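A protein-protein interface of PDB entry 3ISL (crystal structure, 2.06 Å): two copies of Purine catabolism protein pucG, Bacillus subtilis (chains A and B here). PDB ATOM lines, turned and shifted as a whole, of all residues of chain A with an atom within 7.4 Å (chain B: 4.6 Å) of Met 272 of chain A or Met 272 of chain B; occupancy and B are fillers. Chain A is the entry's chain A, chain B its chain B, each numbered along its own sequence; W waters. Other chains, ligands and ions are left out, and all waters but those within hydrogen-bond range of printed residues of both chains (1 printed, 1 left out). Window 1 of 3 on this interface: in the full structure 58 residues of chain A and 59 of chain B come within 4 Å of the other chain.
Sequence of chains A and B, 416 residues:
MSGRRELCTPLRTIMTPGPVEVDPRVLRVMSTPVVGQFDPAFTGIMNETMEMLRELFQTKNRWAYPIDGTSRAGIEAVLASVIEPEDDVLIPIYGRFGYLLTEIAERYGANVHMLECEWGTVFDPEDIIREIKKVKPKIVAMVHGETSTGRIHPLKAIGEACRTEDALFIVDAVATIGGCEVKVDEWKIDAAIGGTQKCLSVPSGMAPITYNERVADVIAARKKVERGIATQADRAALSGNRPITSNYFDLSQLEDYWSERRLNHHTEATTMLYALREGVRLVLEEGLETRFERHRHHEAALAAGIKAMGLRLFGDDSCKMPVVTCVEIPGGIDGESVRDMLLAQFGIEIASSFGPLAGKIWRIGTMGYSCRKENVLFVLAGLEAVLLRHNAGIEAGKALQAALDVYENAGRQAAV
OE1 of Glu 268 of chain A sits close to OD2 of Asp 68 of chain A, 2.5 Å away. The side-chain carboxylate (OD1) of Asp 68 of chain A sits at hydrogen-bond distance from the backbone NH (N) of Ala 269 of chain A (3.1 Å). The side-chain hydroxyl (OG1) of Thr 196 of chain A lies within hydrogen-bond range of the backbone carbonyl oxygen (O) of Pro 203 of chain A, at 3.2 Å.
Among the printed residues, merely in contact across the chains: Ala 269 of chain A with Ser 204 of chain B (3.3 Å), Ser 204 of chain A with Ala 269 of chain B (3.3 Å), Pro 203 of chain A with Thr 271 of chain B (3.4 Å), Thr 271 of chain A with Pro 203 of chain B (3.5 Å), Glu 268 of chain A with Ser 204 of chain B (3.5 Å), Ser 204 of chain A with Thr 270 of chain B (3.6 Å), Met 30 of chain A with Thr 271 of chain B (3.8 Å) and Met 272 of chain A with Met 272 of chain B (3.9 Å).
Of the printed residues of chain B, Pro 203 of chain A touches Thr 271 (3.4 Å). Of the printed residues of chain B, Ala 269 of chain A touches Ser 204. Leu 273 of chain A touches none of the printed residues of chain B. Of chain A, only Met 272 (3.9 Å) comes within 4 Å of Met 272 of chain B. The nearest printed residue of chain B that does not touch Met 272 of chain A is Thr 271 of chain B (5.2 Å). The nearest printed residue of chain B that does not touch Pro 203 of chain A is Thr 270 of chain B (4.01 Å).
Of the 21 printed residues of chain A, 7 touch a printed residue of chain B. Printed residues of chain A that touch a printed residue of chain B: Met 30, Pro 203, Ser 204, Glu 268, Ala 269, Thr 271 and Met 272. Of the 13 printed residues of chain B, 6 touch a printed residue of chain A. Printed residues of chain B that touch a printed residue of chain A: Pro 203, Ser 204, Ala 269, Thr 270, Thr 271 and Met 272. Hydrophobic or aromatic side chains of chain B within 4 Å of the printed part of chain A: Pro 203, Ala 269 and Met 272. Among the printed residues, 8 pairs touch across the chains.
Pro 203 of chain A touches Thr 271 of chain B, and with the chains exchanged Thr 271 of chain A touches Pro 203 of chain B. Ser 204 of chain A touches Ala 269 of chain B, and with the chains exchanged Ala 269 of chain A touches Ser 204 of chain B. Ser 204 of chain A touches Thr 270 of chain B, but with the chains exchanged Thr 270 of chain A does not touch Ser 204 of chain B (4.3 Å). Met 272 of chain A touches its own counterpart, Met 272 of chain B. Of the 8 pairs that touch across the chains among the printed residues, 5 have their exchanged pair printed and touching as well.
Water W1 lies within hydrogen-bond range of O of Ser 204 of chain A (2.7 Å), N of Met 272 of chain B (3.1 Å), N of Thr 271 of chain B (3.4 Å) and SD of Met 272 of chain A (3.7 Å).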
ATOM      1  N   MET A  30      11.916  20.498  23.360  1.00  0.00           N
ATOM      2  CA  MET A  30      12.115  20.757  21.896  1.00  0.00           C
ATOM      3  C   MET A  30      10.928  20.180  21.084  1.00  0.00           C
ATOM      4  O   MET A  30      10.787  20.453  19.906  1.00  0.00           O
ATOM      5  CB  MET A  30      13.470  20.216  21.451  1.00  0.00           C
ATOM      6  CG  MET A  30      14.585  21.088  22.049  1.00  0.00           C
ATOM      7  SD  MET A  30      16.160  20.813  21.221  1.00  0.00           S
ATOM      8  CE  MET A  30      16.614  19.266  22.002  1.00  0.00           C
ATOM      9  N   PHE A  42       7.457  35.176  21.600  1.00  0.00           N
ATOM     10  CA  PHE A  42       8.840  34.896  21.231  1.00  0.00           C
ATOM     11  C   PHE A  42       9.737  36.070  21.684  1.00  0.00           C
ATOM     12  O   PHE A  42      10.813  35.867  22.191  1.00  0.00           O
ATOM     13  CB  PHE A  42       8.988  34.638  19.728  1.00  0.00           C
ATOM     14  CG  PHE A  42      10.255  33.892  19.342  1.00  0.00           C
ATOM     15  CD1 PHE A  42      10.476  32.567  19.748  1.00  0.00           C
ATOM     16  CD2 PHE A  42      11.233  34.519  18.604  1.00  0.00           C
ATOM     17  CE1 PHE A  42      11.679  31.879  19.374  1.00  0.00           C
ATOM     18  CE2 PHE A  42      12.389  33.854  18.180  1.00  0.00           C
ATOM     19  CZ  PHE A  42      12.625  32.550  18.575  1.00  0.00           C
ATOM     20  N   PRO A  66      22.106  35.282  21.321  1.00  0.00           N
ATOM     21  CA  PRO A  66      22.739  34.255  20.493  1.00  0.00           C
ATOM     22  C   PRO A  66      22.748  34.611  18.984  1.00  0.00           C
ATOM     23  O   PRO A  66      21.926  35.348  18.524  1.00  0.00           O
ATOM     24  CB  PRO A  66      21.831  33.027  20.691  1.00  0.00           C
ATOM     25  CG  PRO A  66      20.546  33.574  21.045  1.00  0.00           C
ATOM     26  CD  PRO A  66      20.732  34.929  21.697  1.00  0.00           C
ATOM     27  N   ASP A  68      22.704  32.571  15.115  1.00  0.00           N
ATOM     28  CA  ASP A  68      22.162  31.292  14.701  1.00  0.00           C
ATOM     29  C   ASP A  68      23.285  30.732  13.868  1.00  0.00           C
ATOM     30  O   ASP A  68      23.590  31.242  12.798  1.00  0.00           O
ATOM     31  CB  ASP A  68      20.869  31.518  13.893  1.00  0.00           C
ATOM     32  CG  ASP A  68      19.701  31.982  14.753  1.00  0.00           C
ATOM     33  OD1 ASP A  68      18.606  32.253  14.198  1.00  0.00           O
ATOM     34  OD2 ASP A  68      19.910  32.118  15.993  1.00  0.00           O
ATOM     35  N   THR A 196      26.953  26.023  22.514  1.00  0.00           N
ATOM     36  CA  THR A 196      25.883  25.397  23.286  1.00  0.00           C
ATOM     37  C   THR A 196      26.122  23.918  23.632  1.00  0.00           C
ATOM     38  O   THR A 196      25.621  23.449  24.666  1.00  0.00           O
ATOM     39  CB  THR A 196      24.559  25.465  22.484  1.00  0.00           C
ATOM     40  OG1 THR A 196      24.841  25.223  21.095  1.00  0.00           O
ATOM     41  CG2 THR A 196      23.969  26.850  22.573  1.00  0.00           C
ATOM     42  N   VAL A 202      23.355  22.037  25.455  1.00  0.00           N
ATOM     43  CA  VAL A 202      22.280  22.412  24.532  1.00  0.00           C
ATOM     44  C   VAL A 202      22.601  21.949  23.128  1.00  0.00           C
ATOM     45  O   VAL A 202      23.725  22.028  22.746  1.00  0.00           O
ATOM     46  CB  VAL A 202      22.009  23.935  24.654  1.00  0.00           C
ATOM     47  CG1 VAL A 202      21.141  24.494  23.515  1.00  0.00           C
ATOM     48  CG2 VAL A 202      21.417  24.192  26.035  1.00  0.00           C
ATOM     49  N   PRO A 203      21.607  21.427  22.355  1.00  0.00           N
ATOM     50  CA  PRO A 203      21.974  20.954  20.992  1.00  0.00           C
ATOM     51  C   PRO A 203      22.829  21.980  20.262  1.00  0.00           C
ATOM     52  O   PRO A 203      22.545  23.186  20.361  1.00  0.00           O
ATOM     53  CB  PRO A 203      20.618  20.798  20.292  1.00  0.00           C
ATOM     54  CG  PRO A 203      19.760  20.381  21.426  1.00  0.00           C
ATOM     55  CD  PRO A 203      20.185  21.260  22.616  1.00  0.00           C
ATOM     56  N   SER A 204      23.847  21.495  19.525  1.00  0.00           N
ATOM     57  CA  SER A 204      24.803  22.380  18.836  1.00  0.00           C
ATOM     58  C   SER A 204      24.021  23.106  17.782  1.00  0.00           C
ATOM     59  O   SER A 204      22.951  22.628  17.397  1.00  0.00           O
ATOM     60  CB  SER A 204      25.908  21.564  18.205  1.00  0.00           C
ATOM     61  OG  SER A 204      25.299  20.320  17.908  1.00  0.00           O
ATOM     62  N   GLY A 205      24.567  24.210  17.300  1.00  0.00           N
ATOM     63  CA  GLY A 205      23.847  25.043  16.346  1.00  0.00           C
ATOM     64  C   GLY A 205      23.340  26.390  16.841  1.00  0.00           C
ATOM     65  O   GLY A 205      22.509  27.038  16.180  1.00  0.00           O
ATOM     66  N   MET A 206      23.883  26.867  17.979  1.00  0.00           N
ATOM     67  CA  MET A 206      23.741  28.302  18.271  1.00  0.00           C
ATOM     68  C   MET A 206      24.944  28.747  19.025  1.00  0.00           C
ATOM     69  O   MET A 206      25.638  27.890  19.613  1.00  0.00           O
ATOM     70  CB  MET A 206      22.440  28.636  19.017  1.00  0.00           C
ATOM     71  CG  MET A 206      21.337  29.386  18.183  1.00  0.00           C
ATOM     72  SD  MET A 206      20.144  29.644  19.479  1.00  0.00           S
ATOM     73  CE  MET A 206      18.937  30.821  18.875  1.00  0.00           C
ATOM     74  N   GLU A 268      14.826  34.061  13.338  1.00  0.00           N
ATOM     75  CA  GLU A 268      15.410  33.380  14.487  1.00  0.00           C
ATOM     76  C   GLU A 268      15.012  31.857  14.507  1.00  0.00           C
ATOM     77  O   GLU A 268      13.916  31.494  14.017  1.00  0.00           O
ATOM     78  CB  GLU A 268      15.003  34.098  15.794  1.00  0.00           C
ATOM     79  CG  GLU A 268      15.833  33.640  17.029  1.00  0.00           C
ATOM     80  CD  GLU A 268      17.341  33.784  16.809  1.00  0.00           C
ATOM     81  OE1 GLU A 268      18.169  33.108  17.542  1.00  0.00           O
ATOM     82  OE2 GLU A 268      17.698  34.570  15.899  1.00  0.00           O
ATOM     83  N   ALA A 269      15.904  30.999  14.999  1.00  0.00           N
ATOM     84  CA  ALA A 269      15.655  29.589  15.038  1.00  0.00           C
ATOM     85  C   ALA A 269      14.838  29.297  16.296  1.00  0.00           C
ATOM     86  O   ALA A 269      15.406  29.283  17.432  1.00  0.00           O
ATOM     87  CB  ALA A 269      16.938  28.826  15.089  1.00  0.00           C
ATOM     88  N   THR A 270      13.554  29.064  16.091  1.00  0.00           N
ATOM     89  CA  THR A 270      12.572  28.953  17.175  1.00  0.00           C
ATOM     90  C   THR A 270      12.851  27.914  18.201  1.00  0.00           C
ATOM     91  O   THR A 270      12.992  28.245  19.381  1.00  0.00           O
ATOM     92  CB  THR A 270      11.162  28.712  16.674  1.00  0.00           C
ATOM     93  OG1 THR A 270      10.926  29.572  15.547  1.00  0.00           O
ATOM     94  CG2 THR A 270      10.081  28.958  17.927  1.00  0.00           C
ATOM     95  N   THR A 271      13.019  26.670  17.757  1.00  0.00           N
ATOM     96  CA  THR A 271      13.215  25.561  18.633  1.00  0.00           C
ATOM     97  C   THR A 271      14.595  25.639  19.317  1.00  0.00           C
ATOM     98  O   THR A 271      14.722  25.263  20.484  1.00  0.00           O
ATOM     99  CB  THR A 271      13.044  24.223  17.889  1.00  0.00           C
ATOM    100  OG1 THR A 271      11.699  24.111  17.458  1.00  0.00           O
ATOM    101  CG2 THR A 271      13.438  23.041  18.823  1.00  0.00           C
ATOM    102  N   MET A 272      15.619  26.111  18.606  1.00  0.00           N
ATOM    103  CA  MET A 272      16.971  26.197  19.191  1.00  0.00           C
ATOM    104  C   MET A 272      17.013  27.251  20.303  1.00  0.00           C
ATOM    105  O   MET A 272      17.759  27.119  21.243  1.00  0.00           O
ATOM    106  CB  MET A 272      18.061  26.499  18.137  1.00  0.00           C
ATOM    107  CG  MET A 272      18.427  25.241  17.300  1.00  0.00           C
ATOM    108  SD  MET A 272      18.949  23.807  18.315  1.00  0.00           S
ATOM    109  CE  MET A 272      20.290  24.474  19.344  1.00  0.00           C
ATOM    110  N   LEU A 273      16.203  28.285  20.153  1.00  0.00           N
ATOM    111  CA  LEU A 273      16.018  29.300  21.201  1.00  0.00           C
ATOM    112  C   LEU A 273      15.297  28.765  22.438  1.00  0.00           C
ATOM    113  O   LEU A 273      15.725  29.067  23.554  1.00  0.00           O
ATOM    114  CB  LEU A 273      15.240  30.533  20.650  1.00  0.00           C
ATOM    115  CG  LEU A 273      15.192  31.682  21.698  1.00  0.00           C
ATOM    116  CD1 LEU A 273      16.571  32.160  22.017  1.00  0.00           C
ATOM    117  CD2 LEU A 273      14.312  32.865  21.324  1.00  0.00           C
ATOM    118  N   TYR A 274      14.235  27.950  22.250  1.00  0.00           N
ATOM    119  CA  TYR A 274      13.607  27.246  23.352  1.00  0.00           C
ATOM    120  C   TYR A 274      14.686  26.507  24.144  1.00  0.00           C
ATOM    121  O   TYR A 274      14.731  26.583  25.411  1.00  0.00           O
ATOM    122  CB  TYR A 274      12.554  26.189  22.871  1.00  0.00           C
ATOM    123  CG  TYR A 274      11.238  26.717  22.288  1.00  0.00           C
ATOM    124  CD1 TYR A 274      10.852  28.056  22.434  1.00  0.00           C
ATOM    125  CD2 TYR A 274      10.357  25.837  21.624  1.00  0.00           C
ATOM    126  CE1 TYR A 274       9.614  28.509  21.919  1.00  0.00           C
ATOM    127  CE2 TYR A 274       9.175  26.260  21.101  1.00  0.00           C
ATOM    128  CZ  TYR A 274       8.782  27.603  21.252  1.00  0.00           C
ATOM    129  OH  TYR A 274       7.553  28.027  20.680  1.00  0.00           O
ATOM    130  N   ALA A 275      15.501  25.761  23.388  1.00  0.00           N
ATOM    131  CA  ALA A 275      16.510  24.889  23.964  1.00  0.00           C
ATOM    132  C   ALA A 275      17.581  25.698  24.703  1.00  0.00           C
ATOM    133  O   ALA A 275      17.919  25.371  25.801  1.00  0.00           O
ATOM    134  CB  ALA A 275      17.102  23.936  22.913  1.00  0.00           C
ATOM    135  N   LEU A 276      18.038  26.795  24.136  1.00  0.00           N
ATOM    136  CA  LEU A 276      19.008  27.655  24.804  1.00  0.00           C
ATOM    137  C   LEU A 276      18.444  28.268  26.101  1.00  0.00           C
ATOM    138  O   LEU A 276      19.081  28.226  27.176  1.00  0.00           O
ATOM    139  CB  LEU A 276      19.444  28.801  23.827  1.00  0.00           C
ATOM    140  CG  LEU A 276      20.469  29.744  24.393  1.00  0.00           C
ATOM    141  CD1 LEU A 276      21.824  28.987  24.854  1.00  0.00           C
ATOM    142  CD2 LEU A 276      20.780  30.818  23.392  1.00  0.00           C
ATOM    143  N   ARG A 277      17.283  28.890  25.977  1.00  0.00           N
ATOM    144  CA  ARG A 277      16.549  29.380  27.145  1.00  0.00           C
ATOM    145  C   ARG A 277      16.505  28.346  28.275  1.00  0.00           C
ATOM    146  O   ARG A 277      16.954  28.612  29.416  1.00  0.00           O
ATOM    147  CB  ARG A 277      15.149  29.796  26.677  1.00  0.00           C
ATOM    148  CG  ARG A 277      14.316  30.759  27.640  1.00  0.00           C
ATOM    149  CD  ARG A 277      13.554  29.967  28.661  1.00  0.00           C
ATOM    150  NE  ARG A 277      12.671  30.844  29.434  1.00  0.00           N
ATOM    151  CZ  ARG A 277      11.991  30.490  30.517  1.00  0.00           C
ATOM    152  NH1 ARG A 277      12.037  29.222  30.940  1.00  0.00           N
ATOM    153  NH2 ARG A 277      11.226  31.404  31.152  1.00  0.00           N
ATOM    154  N   GLU A 278      16.026  27.131  27.972  1.00  0.00           N
ATOM    155  CA  GLU A 278      15.969  26.127  29.028  1.00  0.00           C
ATOM    156  C   GLU A 278      17.343  25.701  29.521  1.00  0.00           C
ATOM    157  O   GLU A 278      17.505  25.511  30.706  1.00  0.00           O
ATOM    158  CB  GLU A 278      15.118  24.912  28.665  1.00  0.00           C
ATOM    159  CG  GLU A 278      13.685  25.232  28.378  1.00  0.00           C
ATOM    160  CD  GLU A 278      12.895  25.748  29.611  1.00  0.00           C
ATOM    161  OE1 GLU A 278      11.975  25.059  30.108  1.00  0.00           O
ATOM    162  OE2 GLU A 278      13.171  26.872  30.046  1.00  0.00           O
ATOM    163  N   VAL B 202       9.938  22.414   9.025  1.00  0.00           N
ATOM    164  CA  VAL B 202      10.965  21.999   9.975  1.00  0.00           C
ATOM    165  C   VAL B 202      11.451  23.257  10.708  1.00  0.00           C
ATOM    166  O   VAL B 202      11.572  24.299  10.069  1.00  0.00           O
ATOM    167  CB  VAL B 202      12.120  21.353   9.198  1.00  0.00           C
ATOM    168  CG1 VAL B 202      13.431  21.173  10.112  1.00  0.00           C
ATOM    169  CG2 VAL B 202      11.643  20.030   8.579  1.00  0.00           C
ATOM    170  N   PRO B 203      11.781  23.181  12.016  1.00  0.00           N
ATOM    171  CA  PRO B 203      12.151  24.426  12.731  1.00  0.00           C
ATOM    172  C   PRO B 203      13.158  25.279  12.016  1.00  0.00           C
ATOM    173  O   PRO B 203      14.111  24.735  11.420  1.00  0.00           O
ATOM    174  CB  PRO B 203      12.801  23.909  14.020  1.00  0.00           C
ATOM    175  CG  PRO B 203      12.015  22.728  14.282  1.00  0.00           C
ATOM    176  CD  PRO B 203      11.892  22.029  12.914  1.00  0.00           C
ATOM    177  N   SER B 204      12.954  26.608  12.087  1.00  0.00           N
ATOM    178  CA  SER B 204      13.854  27.515  11.372  1.00  0.00           C
ATOM    179  C   SER B 204      15.285  27.234  11.820  1.00  0.00           C
ATOM    180  O   SER B 204      15.489  26.782  12.963  1.00  0.00           O
ATOM    181  CB  SER B 204      13.514  28.995  11.621  1.00  0.00           C
ATOM    182  OG  SER B 204      14.443  29.827  10.889  1.00  0.00           O
ATOM    183  N   GLY B 205      16.240  27.522  10.944  1.00  0.00           N
ATOM    184  CA  GLY B 205      17.645  27.476  11.307  1.00  0.00           C
ATOM    185  C   GLY B 205      18.478  26.406  10.623  1.00  0.00           C
ATOM    186  O   GLY B 205      19.527  26.002  11.128  1.00  0.00           O
ATOM    187  N   MET B 206      18.062  25.998   9.412  1.00  0.00           N
ATOM    188  CA  MET B 206      18.963  25.223   8.600  1.00  0.00           C
ATOM    189  C   MET B 206      18.522  25.523   7.213  1.00  0.00           C
ATOM    190  O   MET B 206      17.378  25.999   7.022  1.00  0.00           O
ATOM    191  CB  MET B 206      18.932  23.712   8.921  1.00  0.00           C
ATOM    192  CG  MET B 206      20.182  23.089   9.682  1.00  0.00           C
ATOM    193  SD  MET B 206      19.838  21.306   9.549  1.00  0.00           S
ATOM    194  CE  MET B 206      21.251  20.473  10.243  1.00  0.00           C
ATOM    195  N   ALA B 269      24.628  20.434  13.519  1.00  0.00           N
ATOM    196  CA  ALA B 269      23.615  20.640  14.507  1.00  0.00           C
ATOM    197  C   ALA B 269      22.770  19.348  14.620  1.00  0.00           C
ATOM    198  O   ALA B 269      21.890  19.083  13.764  1.00  0.00           O
ATOM    199  CB  ALA B 269      22.715  21.877  14.144  1.00  0.00           C
ATOM    200  N   THR B 270      23.083  18.559  15.642  1.00  0.00           N
ATOM    201  CA  THR B 270      22.517  17.236  15.952  1.00  0.00           C
ATOM    202  C   THR B 270      20.996  17.168  15.879  1.00  0.00           C
ATOM    203  O   THR B 270      20.431  16.558  14.974  1.00  0.00           O
ATOM    204  CB  THR B 270      22.955  16.834  17.367  1.00  0.00           C
ATOM    205  OG1 THR B 270      22.452  17.824  18.319  1.00  0.00           O
ATOM    206  CG2 THR B 270      24.420  16.850  17.460  1.00  0.00           C
ATOM    207  N   THR B 271      20.308  17.851  16.797  1.00  0.00           N
ATOM    208  CA  THR B 271      18.831  17.860  16.808  1.00  0.00           C
ATOM    209  C   THR B 271      18.236  18.383  15.535  1.00  0.00           C
ATOM    210  O   THR B 271      17.213  17.800  15.022  1.00  0.00           O
ATOM    211  CB  THR B 271      18.336  18.666  17.987  1.00  0.00           C
ATOM    212  OG1 THR B 271      18.870  18.065  19.136  1.00  0.00           O
ATOM    213  CG2 THR B 271      16.845  18.667  18.078  1.00  0.00           C
ATOM    214  N   MET B 272      18.839  19.450  14.981  1.00  0.00           N
ATOM    215  CA  MET B 272      18.279  20.049  13.751  1.00  0.00           C
ATOM    216  C   MET B 272      18.407  19.080  12.567  1.00  0.00           C
ATOM    217  O   MET B 272      17.603  19.088  11.656  1.00  0.00           O
ATOM    218  CB  MET B 272      18.963  21.426  13.447  1.00  0.00           C
ATOM    219  CG  MET B 272      18.503  22.591  14.404  1.00  0.00           C
ATOM    220  SD  MET B 272      16.693  22.918  14.307  1.00  0.00           S
ATOM    221  CE  MET B 272      16.443  23.344  12.557  1.00  0.00           C
ATOM    222  N   LEU B 273      19.470  18.295  12.537  1.00  0.00           N
ATOM    223  CA  LEU B 273      19.606  17.262  11.488  1.00  0.00           C
ATOM    224  C   LEU B 273      18.530  16.179  11.700  1.00  0.00           C
ATOM    225  O   LEU B 273      17.828  15.814  10.749  1.00  0.00           O
ATOM    226  CB  LEU B 273      21.015  16.673  11.469  1.00  0.00           C
ATOM    227  CG  LEU B 273      21.117  15.703  10.286  1.00  0.00           C
ATOM    228  CD1 LEU B 273      20.790  16.425   8.962  1.00  0.00           C
ATOM    229  CD2 LEU B 273      22.386  15.011  10.212  1.00  0.00           C
ATOM    230  N   TYR B 274      18.287  15.776  12.961  1.00  0.00           N
ATOM    231  CA  TYR B 274      17.217  14.798  13.226  1.00  0.00           C
ATOM    232  C   TYR B 274      15.878  15.340  12.659  1.00  0.00           C
ATOM    233  O   TYR B 274      15.111  14.585  12.020  1.00  0.00           O
ATOM    234  CB  TYR B 274      16.969  14.640  14.738  1.00  0.00           C
ATOM    235  CG  TYR B 274      17.948  13.821  15.524  1.00  0.00           C
ATOM    236  CD1 TYR B 274      18.948  13.027  14.894  1.00  0.00           C
ATOM    237  CD2 TYR B 274      17.850  13.834  16.912  1.00  0.00           C
ATOM    238  CE1 TYR B 274      19.817  12.223  15.685  1.00  0.00           C
ATOM    239  CE2 TYR B 274      18.699  13.110  17.704  1.00  0.00           C
ATOM    240  CZ  TYR B 274      19.665  12.314  17.117  1.00  0.00           C
ATOM    241  OH  TYR B 274      20.417  11.572  17.990  1.00  0.00           O
ATOM    242  N   ALA B 275      15.591  16.630  12.934  1.00  0.00           N
ATOM    243  CA  ALA B 275      14.321  17.241  12.528  1.00  0.00           C
ATOM    244  C   ALA B 275      14.195  17.361  10.979  1.00  0.00           C
ATOM    245  O   ALA B 275      13.110  17.127  10.423  1.00  0.00           O
ATOM    246  CB  ALA B 275      14.118  18.689  13.177  1.00  0.00           C
ATOM    247  N   LEU B 276      15.278  17.748  10.317  1.00  0.00           N
ATOM    248  CA  LEU B 276      15.280  17.848   8.840  1.00  0.00           C
ATOM    249  C   LEU B 276      15.040  16.485   8.168  1.00  0.00           C
ATOM    250  O   LEU B 276      14.262  16.333   7.204  1.00  0.00           O
ATOM    251  CB  LEU B 276      16.610  18.494   8.317  1.00  0.00           C
ATOM    252  CG  LEU B 276      16.722  18.569   6.786  1.00  0.00           C
ATOM    253  CD1 LEU B 276      15.686  19.639   6.135  1.00  0.00           C
ATOM    254  CD2 LEU B 276      18.086  19.011   6.417  1.00  0.00           C
HETATM  255  O   HOH W   1      20.884  21.157  16.612  1.00  0.00           O
